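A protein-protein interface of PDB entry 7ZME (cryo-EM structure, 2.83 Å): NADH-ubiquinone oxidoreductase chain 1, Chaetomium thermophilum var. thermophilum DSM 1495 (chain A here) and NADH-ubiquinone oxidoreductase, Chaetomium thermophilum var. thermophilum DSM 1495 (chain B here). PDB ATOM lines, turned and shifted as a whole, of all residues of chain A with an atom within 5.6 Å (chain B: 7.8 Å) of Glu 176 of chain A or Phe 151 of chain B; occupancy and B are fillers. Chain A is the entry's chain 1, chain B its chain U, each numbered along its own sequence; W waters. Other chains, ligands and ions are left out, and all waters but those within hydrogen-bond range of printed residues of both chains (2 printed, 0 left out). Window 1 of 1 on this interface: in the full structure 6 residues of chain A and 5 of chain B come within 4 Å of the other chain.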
ATOM      1  N   PRO A 100      -1.769 -11.459   1.384  1.00  0.00           N
ATOM      2  CA  PRO A 100      -1.145 -12.512   0.574  1.00  0.00           C
ATOM      3  C   PRO A 100      -1.353 -13.882   1.217  1.00  0.00           C
ATOM      4  O   PRO A 100      -0.702 -14.166   2.184  1.00  0.00           O
ATOM      5  CB  PRO A 100       0.327 -12.104   0.564  1.00  0.00           C
ATOM      6  CG  PRO A 100       0.362 -10.671   1.012  1.00  0.00           C
ATOM      7  CD  PRO A 100      -0.755 -10.597   2.017  1.00  0.00           C
ATOM      8  N   LEU A 171      -5.938 -16.532  -6.844  1.00  0.00           N
ATOM      9  CA  LEU A 171      -6.356 -15.126  -6.617  1.00  0.00           C
ATOM     10  C   LEU A 171      -5.228 -14.308  -5.974  1.00  0.00           C
ATOM     11  O   LEU A 171      -5.061 -13.160  -6.379  1.00  0.00           O
ATOM     12  CB  LEU A 171      -7.629 -15.108  -5.767  1.00  0.00           C
ATOM     13  CG  LEU A 171      -8.957 -15.139  -6.522  1.00  0.00           C
ATOM     14  CD1 LEU A 171      -9.360 -16.563  -6.845  1.00  0.00           C
ATOM     15  CD2 LEU A 171     -10.051 -14.475  -5.705  1.00  0.00           C
ATOM     16  N   THR A 172      -4.439 -14.889  -5.065  1.00  0.00           N
ATOM     17  CA  THR A 172      -3.300 -14.177  -4.417  1.00  0.00           C
ATOM     18  C   THR A 172      -2.226 -13.812  -5.443  1.00  0.00           C
ATOM     19  O   THR A 172      -1.730 -12.691  -5.361  1.00  0.00           O
ATOM     20  CB  THR A 172      -2.692 -14.941  -3.235  1.00  0.00           C
ATOM     21  OG1 THR A 172      -1.627 -14.147  -2.715  1.00  0.00           O
ATOM     22  CG2 THR A 172      -2.148 -16.302  -3.605  1.00  0.00           C
ATOM     23  N   VAL A 173      -1.914 -14.710  -6.379  1.00  0.00           N
ATOM     24  CA  VAL A 173      -0.848 -14.481  -7.391  1.00  0.00           C
ATOM     25  C   VAL A 173      -1.260 -13.368  -8.356  1.00  0.00           C
ATOM     26  O   VAL A 173      -0.381 -12.645  -8.825  1.00  0.00           O
ATOM     27  CB  VAL A 173      -0.434 -15.784  -8.095  1.00  0.00           C
ATOM     28  CG1 VAL A 173       0.740 -15.564  -9.034  1.00  0.00           C
ATOM     29  CG2 VAL A 173      -0.097 -16.869  -7.089  1.00  0.00           C
ATOM     30  N   ILE A 174      -2.555 -13.224  -8.623  1.00  0.00           N
ATOM     31  CA  ILE A 174      -3.026 -12.221  -9.609  1.00  0.00           C
ATOM     32  C   ILE A 174      -2.883 -10.862  -8.943  1.00  0.00           C
ATOM     33  O   ILE A 174      -2.490  -9.920  -9.640  1.00  0.00           O
ATOM     34  CB  ILE A 174      -4.489 -12.531  -9.984  1.00  0.00           C
ATOM     35  CG1 ILE A 174      -4.618 -13.898 -10.662  1.00  0.00           C
ATOM     36  CG2 ILE A 174      -5.108 -11.424 -10.821  1.00  0.00           C
ATOM     37  CD1 ILE A 174      -6.040 -14.360 -10.870  1.00  0.00           C
ATOM     38  N   VAL A 175      -3.117 -10.789  -7.634  1.00  0.00           N
ATOM     39  CA  VAL A 175      -2.951  -9.517  -6.881  1.00  0.00           C
ATOM     40  C   VAL A 175      -1.457  -9.196  -6.817  1.00  0.00           C
ATOM     41  O   VAL A 175      -1.080  -8.032  -7.052  1.00  0.00           O
ATOM     42  CB  VAL A 175      -3.564  -9.615  -5.471  1.00  0.00           C
ATOM     43  CG1 VAL A 175      -3.379  -8.317  -4.704  1.00  0.00           C
ATOM     44  CG2 VAL A 175      -5.031 -10.003  -5.511  1.00  0.00           C
ATOM     45  N   GLU A 176      -0.646 -10.209  -6.532  1.00  0.00           N
ATOM     46  CA  GLU A 176       0.825 -10.048  -6.441  1.00  0.00           C
ATOM     47  C   GLU A 176       1.385  -9.577  -7.786  1.00  0.00           C
ATOM     48  O   GLU A 176       2.337  -8.801  -7.784  1.00  0.00           O
ATOM     49  CB  GLU A 176       1.431 -11.343  -5.898  1.00  0.00           C
ATOM     50  CG  GLU A 176       1.132 -11.577  -4.433  1.00  0.00           C
ATOM     51  CD  GLU A 176       1.734 -10.525  -3.519  1.00  0.00           C
ATOM     52  OE1 GLU A 176       2.734  -9.906  -3.920  1.00  0.00           O
ATOM     53  OE2 GLU A 176       1.200 -10.324  -2.418  1.00  0.00           O
ATOM     54  N   SER A 177       0.834 -10.072  -8.889  1.00  0.00           N
ATOM     55  CA  SER A 177       1.278  -9.675 -10.248  1.00  0.00           C
ATOM     56  C   SER A 177       1.011  -8.185 -10.482  1.00  0.00           C
ATOM     57  O   SER A 177       1.796  -7.559 -11.197  1.00  0.00           O
ATOM     58  CB  SER A 177       0.627 -10.546 -11.280  1.00  0.00           C
ATOM     59  OG  SER A 177       0.974 -11.906 -11.086  1.00  0.00           O
ATOM     60  N   GLN A 178      -0.082  -7.656  -9.934  1.00  0.00           N
ATOM     61  CA  GLN A 178      -0.489  -6.240 -10.125  1.00  0.00           C
ATOM     62  C   GLN A 178       0.401  -5.271  -9.337  1.00  0.00           C
ATOM     63  O   GLN A 178       0.097  -4.078  -9.348  1.00  0.00           O
ATOM     64  CB  GLN A 178      -1.990  -6.113  -9.884  1.00  0.00           C
ATOM     65  CG  GLN A 178      -2.816  -6.977 -10.816  1.00  0.00           C
ATOM     66  CD  GLN A 178      -4.290  -6.710 -10.673  1.00  0.00           C
ATOM     67  OE1 GLN A 178      -4.759  -5.594 -10.862  1.00  0.00           O
ATOM     68  NE2 GLN A 178      -5.035  -7.750 -10.349  1.00  0.00           N
ATOM     69  N   ARG A 179       1.426  -5.763  -8.639  1.00  0.00           N
ATOM     70  CA  ARG A 179       2.419  -4.850  -8.012  1.00  0.00           C
ATOM     71  C   ARG A 179       3.144  -4.143  -9.163  1.00  0.00           C
ATOM     72  O   ARG A 179       3.589  -3.005  -8.954  1.00  0.00           O
ATOM     73  CB  ARG A 179       3.347  -5.592  -7.044  1.00  0.00           C
ATOM     74  CG  ARG A 179       2.663  -6.087  -5.781  1.00  0.00           C
ATOM     75  CD  ARG A 179       3.635  -6.687  -4.788  1.00  0.00           C
ATOM     76  NE  ARG A 179       2.952  -7.178  -3.603  1.00  0.00           N
ATOM     77  CZ  ARG A 179       2.778  -6.485  -2.486  1.00  0.00           C
ATOM     78  NH1 ARG A 179       3.243  -5.252  -2.394  1.00  0.00           N
ATOM     79  NH2 ARG A 179       2.132  -7.026  -1.469  1.00  0.00           N
ATOM     80  N   ALA A 180       3.291  -4.804 -10.314  1.00  0.00           N
ATOM     81  CA  ALA A 180       3.866  -4.141 -11.507  1.00  0.00           C
ATOM     82  C   ALA A 180       2.948  -2.977 -11.869  1.00  0.00           C
ATOM     83  O   ALA A 180       3.416  -1.833 -11.866  1.00  0.00           O
ATOM     84  CB  ALA A 180       3.910  -5.150 -12.623  1.00  0.00           C
ATOM     85  N   TYR A 255      -5.824  -6.197  -2.593  1.00  0.00           N
ATOM     86  CA  TYR A 255      -5.493  -5.595  -1.309  1.00  0.00           C
ATOM     87  C   TYR A 255      -4.307  -4.640  -1.374  1.00  0.00           C
ATOM     88  O   TYR A 255      -3.916  -4.102  -0.335  1.00  0.00           O
ATOM     89  CB  TYR A 255      -5.209  -6.693  -0.273  1.00  0.00           C
ATOM     90  CG  TYR A 255      -4.221  -7.735  -0.748  1.00  0.00           C
ATOM     91  CD1 TYR A 255      -2.853  -7.502  -0.693  1.00  0.00           C
ATOM     92  CD2 TYR A 255      -4.657  -8.948  -1.254  1.00  0.00           C
ATOM     93  CE1 TYR A 255      -1.954  -8.443  -1.133  1.00  0.00           C
ATOM     94  CE2 TYR A 255      -3.761  -9.900  -1.689  1.00  0.00           C
ATOM     95  CZ  TYR A 255      -2.412  -9.639  -1.633  1.00  0.00           C
ATOM     96  OH  TYR A 255      -1.522 -10.582  -2.073  1.00  0.00           O
ATOM     97  N   LEU A 256      -3.727  -4.418  -2.551  1.00  0.00           N
ATOM     98  CA  LEU A 256      -2.555  -3.562  -2.656  1.00  0.00           C
ATOM     99  C   LEU A 256      -2.882  -2.136  -2.234  1.00  0.00           C
ATOM    100  O   LEU A 256      -3.982  -1.630  -2.462  1.00  0.00           O
ATOM    101  CB  LEU A 256      -2.012  -3.565  -4.084  1.00  0.00           C
ATOM    102  CG  LEU A 256      -1.350  -4.843  -4.597  1.00  0.00           C
ATOM    103  CD1 LEU A 256      -0.668  -4.568  -5.911  1.00  0.00           C
ATOM    104  CD2 LEU A 256      -0.371  -5.404  -3.590  1.00  0.00           C
ATOM    105  N   LEU A 378       5.170 -15.740  -7.064  1.00  0.00           N
ATOM    106  CA  LEU A 378       4.499 -14.672  -6.284  1.00  0.00           C
ATOM    107  C   LEU A 378       3.364 -15.286  -5.451  1.00  0.00           C
ATOM    108  O   LEU A 378       3.278 -14.939  -4.263  1.00  0.00           O
ATOM    109  CB  LEU A 378       3.982 -13.609  -7.260  1.00  0.00           C
ATOM    110  CG  LEU A 378       5.030 -12.954  -8.158  1.00  0.00           C
ATOM    111  CD1 LEU A 378       4.391 -11.927  -9.075  1.00  0.00           C
ATOM    112  CD2 LEU A 378       6.124 -12.301  -7.333  1.00  0.00           C
ATOM    113  N   GLN B 108      11.133 -15.268  -0.017  1.00  0.00           N
ATOM    114  CA  GLN B 108      11.250 -14.599  -1.334  1.00  0.00           C
ATOM    115  C   GLN B 108      12.491 -13.709  -1.279  1.00  0.00           C
ATOM    116  O   GLN B 108      12.534 -12.840  -0.407  1.00  0.00           O
ATOM    117  CB  GLN B 108       9.932 -13.889  -1.623  1.00  0.00           C
ATOM    118  CG  GLN B 108       8.779 -14.860  -1.822  1.00  0.00           C
ATOM    119  CD  GLN B 108       7.427 -14.201  -1.938  1.00  0.00           C
ATOM    120  OE1 GLN B 108       6.431 -14.844  -2.258  1.00  0.00           O
ATOM    121  NE2 GLN B 108       7.381 -12.907  -1.682  1.00  0.00           N
ATOM    122  N   TRP B 110      13.698 -11.316  -3.121  1.00  0.00           N
ATOM    123  CA  TRP B 110      13.498  -9.886  -3.454  1.00  0.00           C
ATOM    124  C   TRP B 110      12.921  -9.118  -2.265  1.00  0.00           C
ATOM    125  O   TRP B 110      12.805  -7.895  -2.376  1.00  0.00           O
ATOM    126  CB  TRP B 110      12.636  -9.764  -4.706  1.00  0.00           C
ATOM    127  CG  TRP B 110      11.234 -10.270  -4.570  1.00  0.00           C
ATOM    128  CD1 TRP B 110      10.145  -9.569  -4.141  1.00  0.00           C
ATOM    129  CD2 TRP B 110      10.756 -11.582  -4.909  1.00  0.00           C
ATOM    130  NE1 TRP B 110       9.028 -10.360  -4.173  1.00  0.00           N
ATOM    131  CE2 TRP B 110       9.372 -11.598  -4.644  1.00  0.00           C
ATOM    132  CE3 TRP B 110      11.360 -12.740  -5.410  1.00  0.00           C
ATOM    133  CZ2 TRP B 110       8.587 -12.727  -4.861  1.00  0.00           C
ATOM    134  CZ3 TRP B 110      10.583 -13.855  -5.622  1.00  0.00           C
ATOM    135  CH2 TRP B 110       9.217 -13.848  -5.348  1.00  0.00           C
ATOM    136  N   GLN B 111      12.532  -9.821  -1.204  1.00  0.00           N
ATOM    137  CA  GLN B 111      11.878  -9.153  -0.058  1.00  0.00           C
ATOM    138  C   GLN B 111      12.902  -8.940   1.051  1.00  0.00           C
ATOM    139  O   GLN B 111      12.525  -8.384   2.088  1.00  0.00           O
ATOM    140  CB  GLN B 111      10.727 -10.024   0.439  1.00  0.00           C
ATOM    141  CG  GLN B 111       9.693 -10.376  -0.618  1.00  0.00           C
ATOM    142  CD  GLN B 111       8.617  -9.327  -0.733  1.00  0.00           C
ATOM    143  OE1 GLN B 111       8.773  -8.202  -0.271  1.00  0.00           O
ATOM    144  NE2 GLN B 111       7.510  -9.688  -1.357  1.00  0.00           N
ATOM    145  N   VAL B 143      18.775  -8.644 -11.634  1.00  0.00           N
ATOM    146  CA  VAL B 143      17.619  -8.347 -10.734  1.00  0.00           C
ATOM    147  C   VAL B 143      18.041  -8.310  -9.257  1.00  0.00           C
ATOM    148  O   VAL B 143      17.429  -7.548  -8.497  1.00  0.00           O
ATOM    149  CB  VAL B 143      16.417  -9.278 -11.004  1.00  0.00           C
ATOM    150  CG1 VAL B 143      16.617 -10.664 -10.411  1.00  0.00           C
ATOM    151  CG2 VAL B 143      15.106  -8.667 -10.539  1.00  0.00           C
ATOM    152  N   ARG B 148      15.753  -0.908  -6.882  1.00  0.00           N
ATOM    153  CA  ARG B 148      14.298  -0.919  -6.650  1.00  0.00           C
ATOM    154  C   ARG B 148      13.751  -2.307  -6.957  1.00  0.00           C
ATOM    155  O   ARG B 148      14.079  -2.855  -8.029  1.00  0.00           O
ATOM    156  CB  ARG B 148      13.656   0.106  -7.577  1.00  0.00           C
ATOM    157  CG  ARG B 148      14.111   1.536  -7.327  1.00  0.00           C
ATOM    158  CD  ARG B 148      13.150   2.544  -7.928  1.00  0.00           C
ATOM    159  NE  ARG B 148      11.789   2.335  -7.453  1.00  0.00           N
ATOM    160  CZ  ARG B 148      11.269   2.901  -6.371  1.00  0.00           C
ATOM    161  NH1 ARG B 148      10.020   2.644  -6.025  1.00  0.00           N
ATOM    162  NH2 ARG B 148      11.998   3.724  -5.639  1.00  0.00           N
ATOM    163  N   GLN B 149      12.971  -2.866  -6.039  1.00  0.00           N
ATOM    164  CA  GLN B 149      12.321  -4.154  -6.337  1.00  0.00           C
ATOM    165  C   GLN B 149      10.839  -3.867  -6.594  1.00  0.00           C
ATOM    166  O   GLN B 149      10.204  -3.307  -5.711  1.00  0.00           O
ATOM    167  CB  GLN B 149      12.630  -5.154  -5.228  1.00  0.00           C
ATOM    168  CG  GLN B 149      14.110  -5.481  -5.087  1.00  0.00           C
ATOM    169  CD  GLN B 149      14.729  -6.190  -6.269  1.00  0.00           C
ATOM    170  OE1 GLN B 149      15.919  -6.054  -6.534  1.00  0.00           O
ATOM    171  NE2 GLN B 149      13.936  -6.972  -6.980  1.00  0.00           N
ATOM    172  N   ILE B 150      10.297  -4.297  -7.731  1.00  0.00           N
ATOM    173  CA  ILE B 150       8.893  -3.920  -8.059  1.00  0.00           C
ATOM    174  C   ILE B 150       7.931  -4.824  -7.283  1.00  0.00           C
ATOM    175  O   ILE B 150       6.806  -4.374  -7.007  1.00  0.00           O
ATOM    176  CB  ILE B 150       8.672  -4.110  -9.576  1.00  0.00           C
ATOM    177  CG1 ILE B 150       9.686  -3.332 -10.417  1.00  0.00           C
ATOM    178  CG2 ILE B 150       7.242  -3.790  -9.984  1.00  0.00           C
ATOM    179  CD1 ILE B 150       9.472  -3.478 -11.902  1.00  0.00           C
ATOM    180  N   PHE B 151       8.373  -6.014  -6.875  1.00  0.00           N
ATOM    181  CA  PHE B 151       7.444  -6.968  -6.220  1.00  0.00           C
ATOM    182  C   PHE B 151       7.694  -6.994  -4.715  1.00  0.00           C
ATOM    183  O   PHE B 151       6.997  -7.747  -4.012  1.00  0.00           O
ATOM    184  CB  PHE B 151       7.457  -8.315  -6.942  1.00  0.00           C
ATOM    185  CG  PHE B 151       6.980  -8.234  -8.368  1.00  0.00           C
ATOM    186  CD1 PHE B 151       5.626  -8.230  -8.663  1.00  0.00           C
ATOM    187  CD2 PHE B 151       7.882  -8.134  -9.413  1.00  0.00           C
ATOM    188  CE1 PHE B 151       5.183  -8.144  -9.972  1.00  0.00           C
ATOM    189  CE2 PHE B 151       7.438  -8.045 -10.721  1.00  0.00           C
ATOM    190  CZ  PHE B 151       6.092  -8.053 -10.999  1.00  0.00           C
ATOM    191  N   ALA B 152       8.627  -6.167  -4.238  1.00  0.00           N
ATOM    192  CA  ALA B 152       8.925  -6.094  -2.786  1.00  0.00           C
ATOM    193  C   ALA B 152       7.847  -5.280  -2.081  1.00  0.00           C
ATOM    194  O   ALA B 152       7.607  -4.148  -2.519  1.00  0.00           O
ATOM    195  CB  ALA B 152      10.282  -5.498  -2.549  1.00  0.00           C
ATOM    196  N   HIS B 153       7.252  -5.830  -1.023  1.00  0.00           N
ATOM    197  CA  HIS B 153       6.141  -5.136  -0.329  1.00  0.00           C
ATOM    198  C   HIS B 153       6.621  -3.846   0.328  1.00  0.00           C
ATOM    199  O   HIS B 153       5.811  -2.919   0.432  1.00  0.00           O
ATOM    200  CB  HIS B 153       5.379  -6.107   0.572  1.00  0.00           C
ATOM    201  CG  HIS B 153       6.207  -6.928   1.495  1.00  0.00           C
ATOM    202  ND1 HIS B 153       7.101  -6.374   2.381  1.00  0.00           N
ATOM    203  CD2 HIS B 153       6.233  -8.259   1.712  1.00  0.00           C
ATOM    204  CE1 HIS B 153       7.672  -7.330   3.080  1.00  0.00           C
ATOM    205  NE2 HIS B 153       7.154  -8.496   2.687  1.00  0.00           N
ATOM    206  N   HIS B 154       7.888  -3.794   0.731  1.00  0.00           N
ATOM    207  CA  HIS B 154       8.476  -2.573   1.328  1.00  0.00           C
ATOM    208  C   HIS B 154       9.572  -2.068   0.398  1.00  0.00           C
ATOM    209  O   HIS B 154      10.413  -2.878  -0.013  1.00  0.00           O
ATOM    210  CB  HIS B 154       9.023  -2.878   2.726  1.00  0.00           C
ATOM    211  CG  HIS B 154       8.004  -3.409   3.676  1.00  0.00           C
ATOM    212  ND1 HIS B 154       8.310  -4.363   4.626  1.00  0.00           N
ATOM    213  CD2 HIS B 154       6.691  -3.130   3.828  1.00  0.00           C
ATOM    214  CE1 HIS B 154       7.230  -4.647   5.323  1.00  0.00           C
ATOM    215  NE2 HIS B 154       6.221  -3.907   4.849  1.00  0.00           N
ATOM    216  N   ILE B 156      12.989  -0.366  -1.034  1.00  0.00           N
ATOM    217  CA  ILE B 156      14.373  -0.513  -0.502  1.00  0.00           C
ATOM    218  C   ILE B 156      14.849   0.884  -0.164  1.00  0.00           C
ATOM    219  O   ILE B 156      14.739   1.757  -1.024  1.00  0.00           O
ATOM    220  CB  ILE B 156      15.314  -1.258  -1.484  1.00  0.00           C
ATOM    221  CG1 ILE B 156      15.022  -2.760  -1.533  1.00  0.00           C
ATOM    222  CG2 ILE B 156      16.770  -1.006  -1.137  1.00  0.00           C
ATOM    223  CD1 ILE B 156      13.769  -3.128  -2.276  1.00  0.00           C
HETATM  224  O   HOH W   1       5.397  -4.058  -3.773  1.00  0.00           O
HETATM  225  O   HOH W   2       5.427 -10.520  -4.317  1.00  0.00           O
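Of chain B, only Phe 151 (3.5 Å) comes within 4 Å of Glu 176 of chain A.
Phe 151 of chain B touches just these residues of chain A: Glu 176, Ser 177, Arg 179, Ala 180 and Leu 378.
Of the printed residues of chain A, Gln 108 of chain B touches Leu 378.
Of the printed residues of chain B, Ser 177 of chain A touches Phe 151.
Of the printed residues of chain B, Leu 378 of chain A touches Gln 108, Trp 110 and Phe 151.
Of the printed residues of chain A, Trp 110 of chain B touches Leu 378 (3.5 Å).
Leu 256 of chain A touches none of the printed residues of chain B.
Ala 152 of chain B touches none of the printed residues of chain A.
Printed residues of chain B that touch a printed residue of chain A: Gln 108, Trp 110, Ile 150, Phe 151 and His 153.
Hydrophobic or aromatic side chains of chain A that line the printed part of chain B: Ala 180 and Leu 378.
Among the printed residues, 10 pairs touch across the chains.
Among the printed residues, no Asp or Glu carboxylate lies within 4 Å of a Lys or Arg side-chain nitrogen of the other chain.
Water W1 bridges O of Ala 152 of chain B and NH1 of Arg 179 of chain A.
Water W2 lies within hydrogen-bond range of the side-chain carboxylate (OE1) of Glu 176 of chain A (2.8 Å) and the backbone carbonyl oxygen (O) of Phe 151 of chain B (3.2 Å).
CD1 of Phe 151 of chain B touches O of Glu 176 of chain A (3.5 Å).
Ser 177 of chain A touches Phe 151 of chain B (O to CE1, 3.6 Å).
Arg 179 of chain A touches Ile 150 of chain B.
CD of Arg 179 of chain A touches O of Phe 151 of chain B, at 3.6 Å.
NH1 of Arg 179 of chain A touches CA of His 153 of chain B (3.6 Å).
Ile 150 of chain B touches Ala 180 of chain A (CG2 to CA, 3.7 Å).
N of Ala 180 of chain A touches CE1 of Phe 151 of chain B, at 3.9 Å.
O of Leu 378 of chain A touches OE1 of Gln 108 of chain B (3.7 Å).
Trp 110 of chain B touches Leu 378 of chain A (CZ2 to CD2, 3.5 Å).
Leu 378 of chain A touches Phe 151 of chain B.
The side-chain carboxylate of Glu 176 of chain A lies within salt-bridge range of the guanidinium group of Arg 179 of chain A.
The side-chain amide nitrogen of Gln 108 of chain B lies close to the side-chain amide nitrogen of Gln 111 of chain B (3.2 Å).
NE1 of Trp 110 of chain B lies close to NE2 of Gln 111 of chain B.
O of Phe 151 of chain B lies within hydrogen-bond range of NE1 of Trp 110 of chain B.
NE2 of Gln 111 of chain B is in hydrogen-bond range of O of Phe 151 of chain B (3.3 Å).
ND1 of His 154 of chain B sits at hydrogen-bond distance from ND1 of His 153 of chain B, 3.2 Å away.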
